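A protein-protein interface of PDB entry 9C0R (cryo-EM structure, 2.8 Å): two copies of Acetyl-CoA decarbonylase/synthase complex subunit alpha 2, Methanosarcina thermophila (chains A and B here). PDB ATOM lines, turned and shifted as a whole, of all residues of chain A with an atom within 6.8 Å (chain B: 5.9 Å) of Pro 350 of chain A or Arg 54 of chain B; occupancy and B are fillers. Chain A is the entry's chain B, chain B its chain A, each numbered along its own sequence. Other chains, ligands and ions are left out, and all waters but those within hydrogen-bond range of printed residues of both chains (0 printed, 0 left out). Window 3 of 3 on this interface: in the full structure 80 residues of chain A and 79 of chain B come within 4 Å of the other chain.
No position is printed for both chains. Of the 10 pairs that touch across the chains among the printed residues, none has its exchanged pair printed and touching as well.
Of chain B, only Arg 54 comes within 4 Å of Pro 350 of chain A. Of chain A, only Met 346, Leu 349, Pro 350 and Asp 351 come within 4 Å of Arg 54 of chain B. Of the printed residues of chain A, Ala 51 of chain B touches Met 346. Of the printed residues of chain B, Leu 349 of chain A touches Arg 54. Val 373 of chain A touches none of the printed residues of chain B. The nearest printed residue of chain B that does not touch Pro 350 of chain A is Phe 58 of chain B (6.3 Å). The nearest printed residue of chain A that does not touch Ile 190 of chain B is Tyr 347 of chain A (5.7 Å).
Among the printed residues, pairs that only touch across the chains: Met 346 of chain A with Ala 50 of chain B (3.9 Å), Met 346 of chain A with Ala 51 of chain B (3.6 Å), Met 346 of chain A with Asp 191 of chain B (3.4 Å), Gly 348 of chain A with Ile 190 of chain B (3.6 Å), Pro 350 of chain A with Arg 54 of chain B (3.97 Å) and Asp 351 of chain A with Arg 54 of chain B (3.7 Å).
The side-chain amide nitrogen (ND2) of Asn 194 of chain B lies within hydrogen-bond range of the backbone carbonyl oxygen (O) of Ala 50 of chain B (2.9 Å). The guanidinium group (NH1) of Arg 54 of chain B lies within salt-bridge range of the side-chain carboxylate (OD1) of Asp 191 of chain B, at 2.9 Å. The backbone carbonyl oxygen (O) of Pro 350 of chain A sits at hydrogen-bond distance from the backbone NH (N) of Val 373 of chain A (2.9 Å). OD1 of Asp 351 of chain A lies within hydrogen-bond range of OG1 of Thr 353 of chain A, at 2.8 Å.
Of the 14 printed residues of chain A, 6 touch a printed residue of chain B. Printed residues of chain A that touch a printed residue of chain B: Met 346, Tyr 347, Gly 348, Leu 349, Pro 350 and Asp 351. Hydrophobic or aromatic side chains of chain A that line the printed part of chain B: Met 346. Of the 14 printed residues of chain B, 5 touch a printed residue of chain A. Among the printed residues, 10 pairs touch across the chains.
NE of Arg 54 of chain B is in hydrogen-bond range of SD of Met 346 of chain A (3.6 Å). The guanidinium group of Arg 54 of chain B sits at hydrogen-bond distance from the backbone carbonyl oxygen of Leu 349 of chain A, at 2.6 Å. The side-chain carboxylate (OD2) of Asp 191 of chain B lies within hydrogen-bond range of the backbone NH (N) of Tyr 347 of chain A (3.5 Å). OD2 of Asp 191 of chain B is in hydrogen-bond range of N of Gly 348 of chain A (2.7 Å).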
ATOM      1  N   MET A 346     -18.366 -13.741 -21.995  1.00  0.00           N
ATOM      2  CA  MET A 346     -17.168 -13.498 -22.783  1.00  0.00           C
ATOM      3  C   MET A 346     -15.911 -14.022 -22.105  1.00  0.00           C
ATOM      4  O   MET A 346     -14.849 -14.042 -22.733  1.00  0.00           O
ATOM      5  CB  MET A 346     -17.030 -12.002 -23.084  1.00  0.00           C
ATOM      6  CG  MET A 346     -17.988 -11.535 -24.162  1.00  0.00           C
ATOM      7  SD  MET A 346     -17.450 -10.070 -25.055  1.00  0.00           S
ATOM      8  CE  MET A 346     -18.498  -8.836 -24.294  1.00  0.00           C
ATOM      9  N   TYR A 347     -16.074 -14.539 -20.882  1.00  0.00           N
ATOM     10  CA  TYR A 347     -15.013 -15.299 -20.163  1.00  0.00           C
ATOM     11  C   TYR A 347     -13.639 -14.626 -20.060  1.00  0.00           C
ATOM     12  O   TYR A 347     -12.685 -15.319 -19.664  1.00  0.00           O
ATOM     13  CB  TYR A 347     -14.898 -16.678 -20.821  1.00  0.00           C
ATOM     14  CG  TYR A 347     -14.938 -17.853 -19.878  1.00  0.00           C
ATOM     15  CD1 TYR A 347     -16.036 -18.088 -19.069  1.00  0.00           C
ATOM     16  CD2 TYR A 347     -13.879 -18.740 -19.805  1.00  0.00           C
ATOM     17  CE1 TYR A 347     -16.079 -19.170 -18.206  1.00  0.00           C
ATOM     18  CE2 TYR A 347     -13.903 -19.825 -18.946  1.00  0.00           C
ATOM     19  CZ  TYR A 347     -15.007 -20.042 -18.144  1.00  0.00           C
ATOM     20  OH  TYR A 347     -15.031 -21.109 -17.299  1.00  0.00           O
ATOM     21  N   GLY A 348     -13.538 -13.334 -20.348  1.00  0.00           N
ATOM     22  CA  GLY A 348     -12.248 -12.680 -20.298  1.00  0.00           C
ATOM     23  C   GLY A 348     -11.305 -13.054 -21.416  1.00  0.00           C
ATOM     24  O   GLY A 348     -10.129 -12.679 -21.366  1.00  0.00           O
ATOM     25  N   LEU A 349     -11.781 -13.784 -22.417  1.00  0.00           N
ATOM     26  CA  LEU A 349     -10.966 -14.182 -23.548  1.00  0.00           C
ATOM     27  C   LEU A 349     -10.812 -13.027 -24.532  1.00  0.00           C
ATOM     28  O   LEU A 349     -11.629 -12.105 -24.554  1.00  0.00           O
ATOM     29  CB  LEU A 349     -11.596 -15.386 -24.242  1.00  0.00           C
ATOM     30  CG  LEU A 349     -11.815 -16.631 -23.383  1.00  0.00           C
ATOM     31  CD1 LEU A 349     -12.901 -17.502 -23.979  1.00  0.00           C
ATOM     32  CD2 LEU A 349     -10.522 -17.409 -23.237  1.00  0.00           C
ATOM     33  N   PRO A 350      -9.758 -13.043 -25.349  1.00  0.00           N
ATOM     34  CA  PRO A 350      -9.621 -12.013 -26.383  1.00  0.00           C
ATOM     35  C   PRO A 350     -10.739 -12.112 -27.409  1.00  0.00           C
ATOM     36  O   PRO A 350     -11.285 -13.187 -27.665  1.00  0.00           O
ATOM     37  CB  PRO A 350      -8.254 -12.315 -27.009  1.00  0.00           C
ATOM     38  CG  PRO A 350      -7.976 -13.736 -26.657  1.00  0.00           C
ATOM     39  CD  PRO A 350      -8.604 -13.956 -25.322  1.00  0.00           C
ATOM     40  N   ASP A 351     -11.083 -10.967 -27.993  1.00  0.00           N
ATOM     41  CA  ASP A 351     -12.158 -10.879 -28.979  1.00  0.00           C
ATOM     42  C   ASP A 351     -11.536 -10.888 -30.371  1.00  0.00           C
ATOM     43  O   ASP A 351     -11.006  -9.876 -30.834  1.00  0.00           O
ATOM     44  CB  ASP A 351     -13.002  -9.630 -28.752  1.00  0.00           C
ATOM     45  CG  ASP A 351     -14.442  -9.814 -29.189  1.00  0.00           C
ATOM     46  OD1 ASP A 351     -14.743 -10.841 -29.829  1.00  0.00           O
ATOM     47  OD2 ASP A 351     -15.274  -8.932 -28.890  1.00  0.00           O
ATOM     48  N   ARG A 352     -11.607 -12.038 -31.037  1.00  0.00           N
ATOM     49  CA  ARG A 352     -11.104 -12.203 -32.394  1.00  0.00           C
ATOM     50  C   ARG A 352     -12.241 -12.357 -33.399  1.00  0.00           C
ATOM     51  O   ARG A 352     -12.108 -13.083 -34.386  1.00  0.00           O
ATOM     52  CB  ARG A 352     -10.159 -13.400 -32.473  1.00  0.00           C
ATOM     53  CG  ARG A 352      -9.364 -13.652 -31.209  1.00  0.00           C
ATOM     54  CD  ARG A 352      -7.980 -13.038 -31.298  1.00  0.00           C
ATOM     55  NE  ARG A 352      -7.451 -13.089 -32.654  1.00  0.00           N
ATOM     56  CZ  ARG A 352      -6.522 -13.940 -33.067  1.00  0.00           C
ATOM     57  NH1 ARG A 352      -5.994 -14.836 -32.251  1.00  0.00           N
ATOM     58  NH2 ARG A 352      -6.113 -13.891 -34.332  1.00  0.00           N
ATOM     59  N   THR A 353     -13.360 -11.670 -33.158  1.00  0.00           N
ATOM     60  CA  THR A 353     -14.549 -11.858 -33.984  1.00  0.00           C
ATOM     61  C   THR A 353     -14.292 -11.466 -35.433  1.00  0.00           C
ATOM     62  O   THR A 353     -14.714 -12.168 -36.358  1.00  0.00           O
ATOM     63  CB  THR A 353     -15.714 -11.054 -33.407  1.00  0.00           C
ATOM     64  OG1 THR A 353     -16.121 -11.628 -32.160  1.00  0.00           O
ATOM     65  CG2 THR A 353     -16.899 -11.049 -34.366  1.00  0.00           C
ATOM     66  N   ILE A 369      -3.119 -18.343 -26.887  1.00  0.00           N
ATOM     67  CA  ILE A 369      -4.327 -18.052 -26.122  1.00  0.00           C
ATOM     68  C   ILE A 369      -5.050 -19.355 -25.798  1.00  0.00           C
ATOM     69  O   ILE A 369      -4.997 -20.305 -26.591  1.00  0.00           O
ATOM     70  CB  ILE A 369      -5.242 -17.085 -26.892  1.00  0.00           C
ATOM     71  CG1 ILE A 369      -5.434 -17.567 -28.331  1.00  0.00           C
ATOM     72  CG2 ILE A 369      -4.658 -15.684 -26.884  1.00  0.00           C
ATOM     73  CD1 ILE A 369      -6.408 -16.733 -29.131  1.00  0.00           C
ATOM     74  N   PRO A 370      -5.728 -19.450 -24.653  1.00  0.00           N
ATOM     75  CA  PRO A 370      -6.519 -20.646 -24.340  1.00  0.00           C
ATOM     76  C   PRO A 370      -7.889 -20.681 -24.999  1.00  0.00           C
ATOM     77  O   PRO A 370      -8.673 -21.595 -24.726  1.00  0.00           O
ATOM     78  CB  PRO A 370      -6.653 -20.563 -22.813  1.00  0.00           C
ATOM     79  CG  PRO A 370      -6.647 -19.106 -22.528  1.00  0.00           C
ATOM     80  CD  PRO A 370      -5.756 -18.464 -23.560  1.00  0.00           C
ATOM     81  N   GLY A 371      -8.187 -19.717 -25.854  1.00  0.00           N
ATOM     82  CA  GLY A 371      -9.482 -19.644 -26.488  1.00  0.00           C
ATOM     83  C   GLY A 371      -9.720 -18.238 -26.997  1.00  0.00           C
ATOM     84  O   GLY A 371      -8.827 -17.395 -26.993  1.00  0.00           O
ATOM     85  N   CYS A 372     -10.955 -18.005 -27.419  1.00  0.00           N
ATOM     86  CA  CYS A 372     -11.298 -16.704 -27.978  1.00  0.00           C
ATOM     87  C   CYS A 372     -12.805 -16.510 -27.941  1.00  0.00           C
ATOM     88  O   CYS A 372     -13.564 -17.433 -27.647  1.00  0.00           O
ATOM     89  CB  CYS A 372     -10.770 -16.556 -29.409  1.00  0.00           C
ATOM     90  SG  CYS A 372     -11.893 -17.158 -30.688  1.00  0.00           S
ATOM     91  N   VAL A 373     -13.225 -15.284 -28.245  1.00  0.00           N
ATOM     92  CA  VAL A 373     -14.632 -14.921 -28.358  1.00  0.00           C
ATOM     93  C   VAL A 373     -14.949 -14.723 -29.832  1.00  0.00           C
ATOM     94  O   VAL A 373     -14.263 -13.960 -30.522  1.00  0.00           O
ATOM     95  CB  VAL A 373     -14.958 -13.653 -27.548  1.00  0.00           C
ATOM     96  CG1 VAL A 373     -16.452 -13.382 -27.565  1.00  0.00           C
ATOM     97  CG2 VAL A 373     -14.454 -13.780 -26.122  1.00  0.00           C
ATOM     98  N   MET A 374     -15.983 -15.408 -30.315  1.00  0.00           N
ATOM     99  CA  MET A 374     -16.404 -15.336 -31.711  1.00  0.00           C
ATOM    100  C   MET A 374     -17.894 -15.018 -31.733  1.00  0.00           C
ATOM    101  O   MET A 374     -18.727 -15.893 -31.477  1.00  0.00           O
ATOM    102  CB  MET A 374     -16.106 -16.641 -32.444  1.00  0.00           C
ATOM    103  CG  MET A 374     -16.598 -16.678 -33.882  1.00  0.00           C
ATOM    104  SD  MET A 374     -15.952 -15.366 -34.933  1.00  0.00           S
ATOM    105  CE  MET A 374     -14.210 -15.456 -34.544  1.00  0.00           C
ATOM    106  N   THR B  49     -23.556  -2.124 -26.714  1.00  0.00           N
ATOM    107  CA  THR B  49     -23.758  -3.306 -25.888  1.00  0.00           C
ATOM    108  C   THR B  49     -22.450  -3.622 -25.163  1.00  0.00           C
ATOM    109  O   THR B  49     -21.495  -2.844 -25.201  1.00  0.00           O
ATOM    110  CB  THR B  49     -24.245  -4.485 -26.732  1.00  0.00           C
ATOM    111  OG1 THR B  49     -23.318  -4.735 -27.795  1.00  0.00           O
ATOM    112  CG2 THR B  49     -25.614  -4.189 -27.318  1.00  0.00           C
ATOM    113  N   ALA B  50     -22.417  -4.775 -24.491  1.00  0.00           N
ATOM    114  CA  ALA B  50     -21.238  -5.142 -23.712  1.00  0.00           C
ATOM    115  C   ALA B  50     -20.012  -5.309 -24.601  1.00  0.00           C
ATOM    116  O   ALA B  50     -18.913  -4.868 -24.244  1.00  0.00           O
ATOM    117  CB  ALA B  50     -21.506  -6.423 -22.923  1.00  0.00           C
ATOM    118  N   ALA B  51     -20.174  -5.948 -25.760  1.00  0.00           N
ATOM    119  CA  ALA B  51     -19.047  -6.124 -26.667  1.00  0.00           C
ATOM    120  C   ALA B  51     -18.683  -4.839 -27.395  1.00  0.00           C
ATOM    121  O   ALA B  51     -17.555  -4.716 -27.885  1.00  0.00           O
ATOM    122  CB  ALA B  51     -19.353  -7.223 -27.681  1.00  0.00           C
ATOM    123  N   THR B  52     -19.605  -3.883 -27.477  1.00  0.00           N
ATOM    124  CA  THR B  52     -19.340  -2.650 -28.207  1.00  0.00           C
ATOM    125  C   THR B  52     -18.435  -1.705 -27.426  1.00  0.00           C
ATOM    126  O   THR B  52     -17.691  -0.927 -28.031  1.00  0.00           O
ATOM    127  CB  THR B  52     -20.660  -1.958 -28.546  1.00  0.00           C
ATOM    128  OG1 THR B  52     -21.661  -2.949 -28.807  1.00  0.00           O
ATOM    129  CG2 THR B  52     -20.504  -1.103 -29.782  1.00  0.00           C
ATOM    130  N   VAL B  53     -18.473  -1.761 -26.097  1.00  0.00           N
ATOM    131  CA  VAL B  53     -17.700  -0.865 -25.247  1.00  0.00           C
ATOM    132  C   VAL B  53     -16.559  -1.590 -24.547  1.00  0.00           C
ATOM    133  O   VAL B  53     -15.920  -1.015 -23.661  1.00  0.00           O
ATOM    134  CB  VAL B  53     -18.600  -0.159 -24.220  1.00  0.00           C
ATOM    135  CG1 VAL B  53     -19.646   0.686 -24.922  1.00  0.00           C
ATOM    136  CG2 VAL B  53     -19.257  -1.180 -23.297  1.00  0.00           C
ATOM    137  N   ARG B  54     -16.291  -2.844 -24.917  1.00  0.00           N
ATOM    138  CA  ARG B  54     -15.288  -3.648 -24.165  1.00  0.00           C
ATOM    139  C   ARG B  54     -13.866  -3.129 -24.402  1.00  0.00           C
ATOM    140  O   ARG B  54     -13.056  -3.234 -23.467  1.00  0.00           O
ATOM    141  CB  ARG B  54     -15.405  -5.141 -24.500  1.00  0.00           C
ATOM    142  CG  ARG B  54     -14.892  -6.056 -23.397  1.00  0.00           C
ATOM    143  CD  ARG B  54     -15.291  -7.503 -23.607  1.00  0.00           C
ATOM    144  NE  ARG B  54     -14.355  -8.234 -24.447  1.00  0.00           N
ATOM    145  CZ  ARG B  54     -13.594  -9.237 -24.027  1.00  0.00           C
ATOM    146  NH1 ARG B  54     -13.674  -9.653 -22.776  1.00  0.00           N
ATOM    147  NH2 ARG B  54     -12.768  -9.833 -24.866  1.00  0.00           N
ATOM    148  N   ASP B  55     -13.581  -2.588 -25.590  1.00  0.00           N
ATOM    149  CA  ASP B  55     -12.246  -2.055 -25.848  1.00  0.00           C
ATOM    150  C   ASP B  55     -11.969  -0.813 -25.010  1.00  0.00           C
ATOM    151  O   ASP B  55     -10.882  -0.675 -24.432  1.00  0.00           O
ATOM    152  CB  ASP B  55     -12.085  -1.744 -27.335  1.00  0.00           C
ATOM    153  CG  ASP B  55     -11.666  -2.955 -28.142  1.00  0.00           C
ATOM    154  OD1 ASP B  55     -11.364  -4.004 -27.535  1.00  0.00           O
ATOM    155  OD2 ASP B  55     -11.640  -2.859 -29.386  1.00  0.00           O
ATOM    156  N   TRP B  56     -12.936   0.104 -24.932  1.00  0.00           N
ATOM    157  CA  TRP B  56     -12.752   1.309 -24.131  1.00  0.00           C
ATOM    158  C   TRP B  56     -12.637   0.978 -22.647  1.00  0.00           C
ATOM    159  O   TRP B  56     -11.795   1.546 -21.939  1.00  0.00           O
ATOM    160  CB  TRP B  56     -13.900   2.284 -24.394  1.00  0.00           C
ATOM    161  CG  TRP B  56     -13.822   3.567 -23.615  1.00  0.00           C
ATOM    162  CD1 TRP B  56     -14.817   4.132 -22.874  1.00  0.00           C
ATOM    163  CD2 TRP B  56     -12.695   4.447 -23.509  1.00  0.00           C
ATOM    164  NE1 TRP B  56     -14.380   5.301 -22.308  1.00  0.00           N
ATOM    165  CE2 TRP B  56     -13.081   5.519 -22.682  1.00  0.00           C
ATOM    166  CE3 TRP B  56     -11.397   4.432 -24.029  1.00  0.00           C
ATOM    167  CZ2 TRP B  56     -12.216   6.561 -22.362  1.00  0.00           C
ATOM    168  CZ3 TRP B  56     -10.543   5.469 -23.711  1.00  0.00           C
ATOM    169  CH2 TRP B  56     -10.956   6.518 -22.886  1.00  0.00           C
ATOM    170  N   SER B  57     -13.464   0.051 -22.157  1.00  0.00           N
ATOM    171  CA  SER B  57     -13.360  -0.361 -20.762  1.00  0.00           C
ATOM    172  C   SER B  57     -12.014  -1.014 -20.478  1.00  0.00           C
ATOM    173  O   SER B  57     -11.421  -0.787 -19.422  1.00  0.00           O
ATOM    174  CB  SER B  57     -14.496  -1.313 -20.397  1.00  0.00           C
ATOM    175  OG  SER B  57     -15.694  -0.966 -21.064  1.00  0.00           O
ATOM    176  N   PHE B  58     -11.523  -1.839 -21.406  1.00  0.00           N
ATOM    177  CA  PHE B  58     -10.220  -2.468 -21.218  1.00  0.00           C
ATOM    178  C   PHE B  58      -9.103  -1.434 -21.205  1.00  0.00           C
ATOM    179  O   PHE B  58      -8.158  -1.545 -20.417  1.00  0.00           O
ATOM    180  CB  PHE B  58      -9.982  -3.510 -22.308  1.00  0.00           C
ATOM    181  CG  PHE B  58     -10.663  -4.825 -22.049  1.00  0.00           C
ATOM    182  CD1 PHE B  58     -11.436  -5.011 -20.915  1.00  0.00           C
ATOM    183  CD2 PHE B  58     -10.534  -5.872 -22.943  1.00  0.00           C
ATOM    184  CE1 PHE B  58     -12.064  -6.216 -20.678  1.00  0.00           C
ATOM    185  CE2 PHE B  58     -11.159  -7.079 -22.712  1.00  0.00           C
ATOM    186  CZ  PHE B  58     -11.925  -7.251 -21.579  1.00  0.00           C
ATOM    187  N   THR B  59      -9.196  -0.418 -22.069  1.00  0.00           N
ATOM    188  CA  THR B  59      -8.226   0.673 -22.035  1.00  0.00           C
ATOM    189  C   THR B  59      -8.254   1.388 -20.689  1.00  0.00           C
ATOM    190  O   THR B  59      -7.201   1.703 -20.122  1.00  0.00           O
ATOM    191  CB  THR B  59      -8.502   1.656 -23.176  1.00  0.00           C
ATOM    192  OG1 THR B  59      -7.903   1.172 -24.383  1.00  0.00           O
ATOM    193  CG2 THR B  59      -7.932   3.028 -22.861  1.00  0.00           C
ATOM    194  N   ILE B 190     -13.140  -8.978 -14.983  1.00  0.00           N
ATOM    195  CA  ILE B 190     -12.954  -7.834 -15.872  1.00  0.00           C
ATOM    196  C   ILE B 190     -14.172  -7.638 -16.770  1.00  0.00           C
ATOM    197  O   ILE B 190     -14.563  -6.504 -17.070  1.00  0.00           O
ATOM    198  CB  ILE B 190     -11.657  -8.000 -16.684  1.00  0.00           C
ATOM    199  CG1 ILE B 190     -11.604  -9.385 -17.331  1.00  0.00           C
ATOM    200  CG2 ILE B 190     -10.446  -7.785 -15.797  1.00  0.00           C
ATOM    201  CD1 ILE B 190     -11.842  -9.376 -18.815  1.00  0.00           C
ATOM    202  N   ASP B 191     -14.793  -8.733 -17.215  1.00  0.00           N
ATOM    203  CA  ASP B 191     -16.012  -8.601 -18.005  1.00  0.00           C
ATOM    204  C   ASP B 191     -17.170  -8.088 -17.160  1.00  0.00           C
ATOM    205  O   ASP B 191     -18.009  -7.324 -17.654  1.00  0.00           O
ATOM    206  CB  ASP B 191     -16.362  -9.937 -18.656  1.00  0.00           C
ATOM    207  CG  ASP B 191     -15.719 -10.105 -20.016  1.00  0.00           C
ATOM    208  OD1 ASP B 191     -15.701  -9.130 -20.794  1.00  0.00           O
ATOM    209  OD2 ASP B 191     -15.225 -11.212 -20.309  1.00  0.00           O
ATOM    210  N   ASN B 194     -16.615  -4.414 -17.138  1.00  0.00           N
ATOM    211  CA  ASN B 194     -17.078  -3.825 -18.393  1.00  0.00           C
ATOM    212  C   ASN B 194     -18.597  -3.670 -18.399  1.00  0.00           C
ATOM    213  O   ASN B 194     -19.133  -2.622 -18.789  1.00  0.00           O
ATOM    214  CB  ASN B 194     -16.615  -4.689 -19.568  1.00  0.00           C
ATOM    215  CG  ASN B 194     -17.180  -4.225 -20.895  1.00  0.00           C
ATOM    216  OD1 ASN B 194     -16.946  -3.098 -21.322  1.00  0.00           O
ATOM    217  ND2 ASN B 194     -17.931  -5.098 -21.555  1.00  0.00           N
